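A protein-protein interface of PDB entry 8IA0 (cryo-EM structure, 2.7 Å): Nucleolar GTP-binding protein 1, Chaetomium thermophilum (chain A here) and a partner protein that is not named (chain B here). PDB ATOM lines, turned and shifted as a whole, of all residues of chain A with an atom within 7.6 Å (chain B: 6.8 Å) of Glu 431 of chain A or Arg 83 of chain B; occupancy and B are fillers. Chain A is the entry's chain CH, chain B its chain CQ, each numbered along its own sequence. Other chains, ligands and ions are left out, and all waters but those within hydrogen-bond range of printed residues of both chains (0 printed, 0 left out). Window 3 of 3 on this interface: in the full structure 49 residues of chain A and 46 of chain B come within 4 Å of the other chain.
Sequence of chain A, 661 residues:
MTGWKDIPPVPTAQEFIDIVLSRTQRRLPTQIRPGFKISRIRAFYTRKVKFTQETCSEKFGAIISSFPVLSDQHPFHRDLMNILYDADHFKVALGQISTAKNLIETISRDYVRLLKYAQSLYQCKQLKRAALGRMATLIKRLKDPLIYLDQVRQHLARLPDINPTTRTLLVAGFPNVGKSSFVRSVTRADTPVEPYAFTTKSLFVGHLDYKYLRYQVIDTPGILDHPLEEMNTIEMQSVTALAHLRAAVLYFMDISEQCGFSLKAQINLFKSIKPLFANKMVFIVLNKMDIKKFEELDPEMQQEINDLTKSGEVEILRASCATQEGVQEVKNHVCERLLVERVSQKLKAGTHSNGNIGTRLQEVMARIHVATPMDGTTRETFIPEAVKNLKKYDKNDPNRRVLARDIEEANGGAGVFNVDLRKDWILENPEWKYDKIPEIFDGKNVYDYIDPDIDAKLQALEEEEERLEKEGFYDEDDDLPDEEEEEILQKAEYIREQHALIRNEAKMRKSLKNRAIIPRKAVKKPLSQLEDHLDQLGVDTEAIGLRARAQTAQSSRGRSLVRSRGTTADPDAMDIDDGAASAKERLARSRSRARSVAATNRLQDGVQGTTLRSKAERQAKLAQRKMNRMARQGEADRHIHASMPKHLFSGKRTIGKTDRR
The guanidinium group of Arg 83 of chain B lies within salt-bridge range of the side-chain carboxylate of Asp 435 of chain A (2.9 Å).
OH of Tyr 81 of chain B sits close to OD2 of Asp 435 of chain A (3.5 Å).
The indole nitrogen of Trp 432 of chain A lies close to the guanidinium group of Arg 83 of chain B, 3.4 Å away.
The backbone NH (N) of Glu 84 of chain B lies close to the side-chain amide oxygen (OD1) of Asn 82 of chain B, at 3.3 Å.
Leu 427 of chain A touches Tyr 81 of chain B (CD2 to CD2, 3.4 Å).
Arg 83 of chain B touches Glu 431 of chain A.
Tyr 81 of chain B touches Trp 432 of chain A.
Asn 82 of chain B touches Trp 432 of chain A (OD1 to CH2, 3.0 Å).
Trp 432 of chain A touches Glu 84 of chain B.
Pro 438 of chain A touches Trp 86 of chain B (CD to CD1, 3.9 Å).
Glu 428 of chain A touches none of the printed residues of chain B.
Glu 431 of chain A touches one residue of chain B.
Of the printed residues of chain B, Asp 435 of chain A touches Tyr 81 and Arg 83.
Of the printed residues of chain A, Asn 82 of chain B touches Trp 432 (3.0 Å).
Arg 83 of chain B touches just these residues of chain A: Glu 431, Trp 432 and Asp 435.
Of the printed residues of chain A, Glu 84 of chain B touches Trp 432 (3.4 Å).
Leu 85 of chain B touches none of the printed residues of chain A.
Printed residues of chain A within 4 Å of Trp 86 of chain B: Pro 438 (3.9 Å).
The nearest printed residue of chain B that does not touch Glu 431 of chain A is Tyr 81 of chain B (7.1 Å).
The nearest residue of chain A that does not touch Arg 83 of chain B is Asn 429 of chain A (5.7 Å).
The nearest printed residue of chain A that does not touch Glu 84 of chain B is Asn 429 of chain A (6.6 Å).
Of the 10 printed residues of chain A, 5 touch a printed residue of chain B.
Printed residues of chain B that touch a printed residue of chain A: Tyr 81, Asn 82, Arg 83, Glu 84 and Trp 86.
Among the printed residues, Asp or Glu carboxylates within 4 Å of a Lys or Arg side-chain nitrogen of the other chain: Asp 435 of chain A with Arg 83 of chain B (2.9 Å).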
ATOM      1  N   LEU A 427     -14.514  17.843  -6.524  1.00  0.00           N
ATOM      2  CA  LEU A 427     -15.779  18.324  -5.990  1.00  0.00           C
ATOM      3  C   LEU A 427     -16.733  17.156  -5.762  1.00  0.00           C
ATOM      4  O   LEU A 427     -16.403  15.989  -5.993  1.00  0.00           O
ATOM      5  CB  LEU A 427     -16.422  19.358  -6.919  1.00  0.00           C
ATOM      6  CG  LEU A 427     -15.900  20.791  -7.075  1.00  0.00           C
ATOM      7  CD1 LEU A 427     -14.421  20.870  -7.389  1.00  0.00           C
ATOM      8  CD2 LEU A 427     -16.711  21.504  -8.142  1.00  0.00           C
ATOM      9  N   GLU A 428     -17.942  17.492  -5.309  1.00  0.00           N
ATOM     10  CA  GLU A 428     -18.958  16.488  -5.015  1.00  0.00           C
ATOM     11  C   GLU A 428     -19.608  15.969  -6.292  1.00  0.00           C
ATOM     12  O   GLU A 428     -19.681  14.756  -6.519  1.00  0.00           O
ATOM     13  CB  GLU A 428     -20.012  17.080  -4.073  1.00  0.00           C
ATOM     14  CG  GLU A 428     -20.715  16.107  -3.108  1.00  0.00           C
ATOM     15  CD  GLU A 428     -19.791  15.316  -2.175  1.00  0.00           C
ATOM     16  OE1 GLU A 428     -18.568  15.219  -2.411  1.00  0.00           O
ATOM     17  OE2 GLU A 428     -20.308  14.782  -1.171  1.00  0.00           O
ATOM     18  N   ASN A 429     -20.094  16.877  -7.137  1.00  0.00           N
ATOM     19  CA  ASN A 429     -20.660  16.507  -8.424  1.00  0.00           C
ATOM     20  C   ASN A 429     -19.671  16.857  -9.521  1.00  0.00           C
ATOM     21  O   ASN A 429     -19.403  18.049  -9.740  1.00  0.00           O
ATOM     22  CB  ASN A 429     -21.985  17.225  -8.652  1.00  0.00           C
ATOM     23  CG  ASN A 429     -22.723  16.715  -9.872  1.00  0.00           C
ATOM     24  OD1 ASN A 429     -22.943  17.453 -10.831  1.00  0.00           O
ATOM     25  ND2 ASN A 429     -23.112  15.447  -9.841  1.00  0.00           N
ATOM     26  N   PRO A 430     -19.095  15.871 -10.213  1.00  0.00           N
ATOM     27  CA  PRO A 430     -18.076  16.175 -11.232  1.00  0.00           C
ATOM     28  C   PRO A 430     -18.529  17.154 -12.302  1.00  0.00           C
ATOM     29  O   PRO A 430     -17.681  17.842 -12.884  1.00  0.00           O
ATOM     30  CB  PRO A 430     -17.780  14.795 -11.842  1.00  0.00           C
ATOM     31  CG  PRO A 430     -18.582  13.786 -10.990  1.00  0.00           C
ATOM     32  CD  PRO A 430     -18.915  14.499  -9.729  1.00  0.00           C
ATOM     33  N   GLU A 431     -19.827  17.238 -12.590  1.00  0.00           N
ATOM     34  CA  GLU A 431     -20.309  18.158 -13.613  1.00  0.00           C
ATOM     35  C   GLU A 431     -20.202  19.618 -13.192  1.00  0.00           C
ATOM     36  O   GLU A 431     -20.391  20.502 -14.033  1.00  0.00           O
ATOM     37  CB  GLU A 431     -21.757  17.818 -13.970  1.00  0.00           C
ATOM     38  CG  GLU A 431     -22.190  18.271 -15.355  1.00  0.00           C
ATOM     39  CD  GLU A 431     -23.672  18.579 -15.429  1.00  0.00           C
ATOM     40  OE1 GLU A 431     -24.422  18.107 -14.548  1.00  0.00           O
ATOM     41  OE2 GLU A 431     -24.087  19.292 -16.366  1.00  0.00           O
ATOM     42  N   TRP A 432     -19.901  19.893 -11.922  1.00  0.00           N
ATOM     43  CA  TRP A 432     -19.805  21.262 -11.435  1.00  0.00           C
ATOM     44  C   TRP A 432     -18.487  21.937 -11.792  1.00  0.00           C
ATOM     45  O   TRP A 432     -18.373  23.154 -11.620  1.00  0.00           O
ATOM     46  CB  TRP A 432     -19.998  21.294  -9.919  1.00  0.00           C
ATOM     47  CG  TRP A 432     -21.405  21.052  -9.509  1.00  0.00           C
ATOM     48  CD1 TRP A 432     -22.514  21.183 -10.286  1.00  0.00           C
ATOM     49  CD2 TRP A 432     -21.862  20.626  -8.223  1.00  0.00           C
ATOM     50  NE1 TRP A 432     -23.637  20.870  -9.563  1.00  0.00           N
ATOM     51  CE2 TRP A 432     -23.263  20.522  -8.293  1.00  0.00           C
ATOM     52  CE3 TRP A 432     -21.222  20.322  -7.019  1.00  0.00           C
ATOM     53  CZ2 TRP A 432     -24.034  20.131  -7.207  1.00  0.00           C
ATOM     54  CZ3 TRP A 432     -21.989  19.933  -5.946  1.00  0.00           C
ATOM     55  CH2 TRP A 432     -23.380  19.840  -6.046  1.00  0.00           C
ATOM     56  N   LYS A 433     -17.495  21.191 -12.264  1.00  0.00           N
ATOM     57  CA  LYS A 433     -16.282  21.817 -12.759  1.00  0.00           C
ATOM     58  C   LYS A 433     -16.588  22.600 -14.031  1.00  0.00           C
ATOM     59  O   LYS A 433     -17.581  22.351 -14.721  1.00  0.00           O
ATOM     60  CB  LYS A 433     -15.202  20.767 -13.013  1.00  0.00           C
ATOM     61  CG  LYS A 433     -15.203  19.637 -11.995  1.00  0.00           C
ATOM     62  CD  LYS A 433     -13.997  18.724 -12.145  1.00  0.00           C
ATOM     63  CE  LYS A 433     -13.736  18.371 -13.595  1.00  0.00           C
ATOM     64  NZ  LYS A 433     -12.480  17.589 -13.750  1.00  0.00           N
ATOM     65  N   TYR A 434     -15.721  23.566 -14.331  1.00  0.00           N
ATOM     66  CA  TYR A 434     -15.934  24.509 -15.431  1.00  0.00           C
ATOM     67  C   TYR A 434     -17.227  25.298 -15.240  1.00  0.00           C
ATOM     68  O   TYR A 434     -17.967  25.556 -16.191  1.00  0.00           O
ATOM     69  CB  TYR A 434     -15.927  23.804 -16.790  1.00  0.00           C
ATOM     70  CG  TYR A 434     -14.873  22.734 -16.924  1.00  0.00           C
ATOM     71  CD1 TYR A 434     -13.549  23.066 -17.155  1.00  0.00           C
ATOM     72  CD2 TYR A 434     -15.203  21.390 -16.829  1.00  0.00           C
ATOM     73  CE1 TYR A 434     -12.582  22.094 -17.281  1.00  0.00           C
ATOM     74  CE2 TYR A 434     -14.241  20.410 -16.952  1.00  0.00           C
ATOM     75  CZ  TYR A 434     -12.933  20.768 -17.178  1.00  0.00           C
ATOM     76  OH  TYR A 434     -11.968  19.796 -17.304  1.00  0.00           O
ATOM     77  N   ASP A 435     -17.503  25.683 -13.998  1.00  0.00           N
ATOM     78  CA  ASP A 435     -18.634  26.536 -13.668  1.00  0.00           C
ATOM     79  C   ASP A 435     -18.142  27.936 -13.335  1.00  0.00           C
ATOM     80  O   ASP A 435     -17.149  28.101 -12.620  1.00  0.00           O
ATOM     81  CB  ASP A 435     -19.429  25.982 -12.484  1.00  0.00           C
ATOM     82  CG  ASP A 435     -20.638  25.182 -12.916  1.00  0.00           C
ATOM     83  OD1 ASP A 435     -21.103  25.377 -14.058  1.00  0.00           O
ATOM     84  OD2 ASP A 435     -21.127  24.363 -12.113  1.00  0.00           O
ATOM     85  N   PRO A 438     -20.247  32.690  -9.149  1.00  0.00           N
ATOM     86  CA  PRO A 438     -20.605  34.100  -8.965  1.00  0.00           C
ATOM     87  C   PRO A 438     -19.737  34.767  -7.911  1.00  0.00           C
ATOM     88  O   PRO A 438     -19.290  34.137  -6.951  1.00  0.00           O
ATOM     89  CB  PRO A 438     -22.071  34.037  -8.521  1.00  0.00           C
ATOM     90  CG  PRO A 438     -22.561  32.726  -9.033  1.00  0.00           C
ATOM     91  CD  PRO A 438     -21.393  31.797  -8.920  1.00  0.00           C
ATOM     92  N   ARG B  80     -15.494  24.345   0.106  1.00  0.00           N
ATOM     93  CA  ARG B  80     -15.435  23.671  -1.183  1.00  0.00           C
ATOM     94  C   ARG B  80     -16.614  24.081  -2.054  1.00  0.00           C
ATOM     95  O   ARG B  80     -17.735  24.252  -1.567  1.00  0.00           O
ATOM     96  CB  ARG B  80     -15.431  22.156  -0.983  1.00  0.00           C
ATOM     97  CG  ARG B  80     -15.116  21.359  -2.233  1.00  0.00           C
ATOM     98  CD  ARG B  80     -14.840  19.907  -1.895  1.00  0.00           C
ATOM     99  NE  ARG B  80     -13.650  19.761  -1.067  1.00  0.00           N
ATOM    100  CZ  ARG B  80     -12.421  19.634  -1.544  1.00  0.00           C
ATOM    101  NH1 ARG B  80     -12.181  19.614  -2.843  1.00  0.00           N
ATOM    102  NH2 ARG B  80     -11.405  19.521  -0.694  1.00  0.00           N
ATOM    103  N   TYR B  81     -16.352  24.253  -3.347  1.00  0.00           N
ATOM    104  CA  TYR B  81     -17.383  24.748  -4.248  1.00  0.00           C
ATOM    105  C   TYR B  81     -18.551  23.774  -4.315  1.00  0.00           C
ATOM    106  O   TYR B  81     -18.370  22.555  -4.349  1.00  0.00           O
ATOM    107  CB  TYR B  81     -16.821  24.981  -5.649  1.00  0.00           C
ATOM    108  CG  TYR B  81     -17.887  25.377  -6.643  1.00  0.00           C
ATOM    109  CD1 TYR B  81     -18.488  26.624  -6.581  1.00  0.00           C
ATOM    110  CD2 TYR B  81     -18.309  24.500  -7.626  1.00  0.00           C
ATOM    111  CE1 TYR B  81     -19.469  26.986  -7.476  1.00  0.00           C
ATOM    112  CE2 TYR B  81     -19.289  24.853  -8.525  1.00  0.00           C
ATOM    113  CZ  TYR B  81     -19.866  26.097  -8.446  1.00  0.00           C
ATOM    114  OH  TYR B  81     -20.841  26.455  -9.344  1.00  0.00           O
ATOM    115  N   ASN B  82     -19.756  24.332  -4.334  1.00  0.00           N
ATOM    116  CA  ASN B  82     -20.983  23.545  -4.361  1.00  0.00           C
ATOM    117  C   ASN B  82     -22.037  24.389  -5.054  1.00  0.00           C
ATOM    118  O   ASN B  82     -22.379  25.468  -4.561  1.00  0.00           O
ATOM    119  CB  ASN B  82     -21.410  23.171  -2.942  1.00  0.00           C
ATOM    120  CG  ASN B  82     -22.555  22.185  -2.909  1.00  0.00           C
ATOM    121  OD1 ASN B  82     -23.219  21.950  -3.914  1.00  0.00           O
ATOM    122  ND2 ASN B  82     -22.790  21.597  -1.744  1.00  0.00           N
ATOM    123  N   ARG B  83     -22.537  23.915  -6.198  1.00  0.00           N
ATOM    124  CA  ARG B  83     -23.460  24.728  -6.984  1.00  0.00           C
ATOM    125  C   ARG B  83     -24.716  25.055  -6.192  1.00  0.00           C
ATOM    126  O   ARG B  83     -25.202  26.191  -6.225  1.00  0.00           O
ATOM    127  CB  ARG B  83     -23.831  24.023  -8.287  1.00  0.00           C
ATOM    128  CG  ARG B  83     -24.643  24.905  -9.223  1.00  0.00           C
ATOM    129  CD  ARG B  83     -25.151  24.155 -10.442  1.00  0.00           C
ATOM    130  NE  ARG B  83     -24.083  23.771 -11.355  1.00  0.00           N
ATOM    131  CZ  ARG B  83     -24.253  22.984 -12.408  1.00  0.00           C
ATOM    132  NH1 ARG B  83     -25.438  22.485 -12.712  1.00  0.00           N
ATOM    133  NH2 ARG B  83     -23.207  22.693 -13.176  1.00  0.00           N
ATOM    134  N   GLU B  84     -25.258  24.071  -5.470  1.00  0.00           N
ATOM    135  CA  GLU B  84     -26.463  24.315  -4.689  1.00  0.00           C
ATOM    136  C   GLU B  84     -26.218  25.362  -3.612  1.00  0.00           C
ATOM    137  O   GLU B  84     -27.057  26.242  -3.394  1.00  0.00           O
ATOM    138  CB  GLU B  84     -26.962  23.009  -4.067  1.00  0.00           C
ATOM    139  CG  GLU B  84     -26.618  21.744  -4.853  1.00  0.00           C
ATOM    140  CD  GLU B  84     -27.387  21.602  -6.163  1.00  0.00           C
ATOM    141  OE1 GLU B  84     -28.027  22.576  -6.615  1.00  0.00           O
ATOM    142  OE2 GLU B  84     -27.350  20.499  -6.745  1.00  0.00           O
ATOM    143  N   LEU B  85     -25.068  25.291  -2.941  1.00  0.00           N
ATOM    144  CA  LEU B  85     -24.764  26.239  -1.873  1.00  0.00           C
ATOM    145  C   LEU B  85     -24.670  27.663  -2.406  1.00  0.00           C
ATOM    146  O   LEU B  85     -25.165  28.606  -1.779  1.00  0.00           O
ATOM    147  CB  LEU B  85     -23.464  25.837  -1.177  1.00  0.00           C
ATOM    148  CG  LEU B  85     -23.006  26.735  -0.031  1.00  0.00           C
ATOM    149  CD1 LEU B  85     -24.072  26.801   1.047  1.00  0.00           C
ATOM    150  CD2 LEU B  85     -21.693  26.233   0.541  1.00  0.00           C
ATOM    151  N   TRP B  86     -24.028  27.842  -3.562  1.00  0.00           N
ATOM    152  CA  TRP B  86     -23.864  29.184  -4.113  1.00  0.00           C
ATOM    153  C   TRP B  86     -25.196  29.759  -4.579  1.00  0.00           C
ATOM    154  O   TRP B  86     -25.460  30.955  -4.413  1.00  0.00           O
ATOM    155  CB  TRP B  86     -22.851  29.166  -5.257  1.00  0.00           C
ATOM    156  CG  TRP B  86     -21.509  29.695  -4.864  1.00  0.00           C
ATOM    157  CD1 TRP B  86     -20.980  30.906  -5.195  1.00  0.00           C
ATOM    158  CD2 TRP B  86     -20.522  29.031  -4.067  1.00  0.00           C
ATOM    159  NE1 TRP B  86     -19.728  31.042  -4.648  1.00  0.00           N
ATOM    160  CE2 TRP B  86     -19.422  29.901  -3.955  1.00  0.00           C
ATOM    161  CE3 TRP B  86     -20.463  27.786  -3.436  1.00  0.00           C
ATOM    162  CZ2 TRP B  86     -18.277  29.568  -3.239  1.00  0.00           C
ATOM    163  CZ3 TRP B  86     -19.325  27.456  -2.727  1.00  0.00           C
ATOM    164  CH2 TRP B  86     -18.248  28.343  -2.633  1.00  0.00           C
ATOM    165  N   GLN B  87     -26.048  28.921  -5.174  1.00  0.00           N
ATOM    166  CA  GLN B  87     -27.334  29.404  -5.665  1.00  0.00           C
ATOM    167  C   GLN B  87     -28.232  29.863  -4.522  1.00  0.00           C
ATOM    168  O   GLN B  87     -28.891  30.905  -4.618  1.00  0.00           O
ATOM    169  CB  GLN B  87     -28.023  28.321  -6.494  1.00  0.00           C
ATOM    170  CG  GLN B  87     -27.293  27.980  -7.779  1.00  0.00           C
ATOM    171  CD  GLN B  87     -27.081  29.189  -8.666  1.00  0.00           C
ATOM    172  OE1 GLN B  87     -28.002  29.971  -8.899  1.00  0.00           O
ATOM    173  NE2 GLN B  87     -25.861  29.351  -9.163  1.00  0.00           N
ATOM    174  N   LYS B  88     -28.275  29.099  -3.428  1.00  0.00           N
ATOM    175  CA  LYS B  88     -29.117  29.500  -2.307  1.00  0.00           C
ATOM    176  C   LYS B  88     -28.503  30.664  -1.545  1.00  0.00           C
ATOM    177  O   LYS B  88     -29.223  31.428  -0.894  1.00  0.00           O
ATOM    178  CB  LYS B  88     -29.363  28.321  -1.365  1.00  0.00           C
ATOM    179  CG  LYS B  88     -28.111  27.613  -0.896  1.00  0.00           C
ATOM    180  CD  LYS B  88     -28.373  26.794   0.355  1.00  0.00           C
ATOM    181  CE  LYS B  88     -29.547  25.845   0.169  1.00  0.00           C
ATOM    182  NZ  LYS B  88     -29.480  25.098  -1.119  1.00  0.00           N
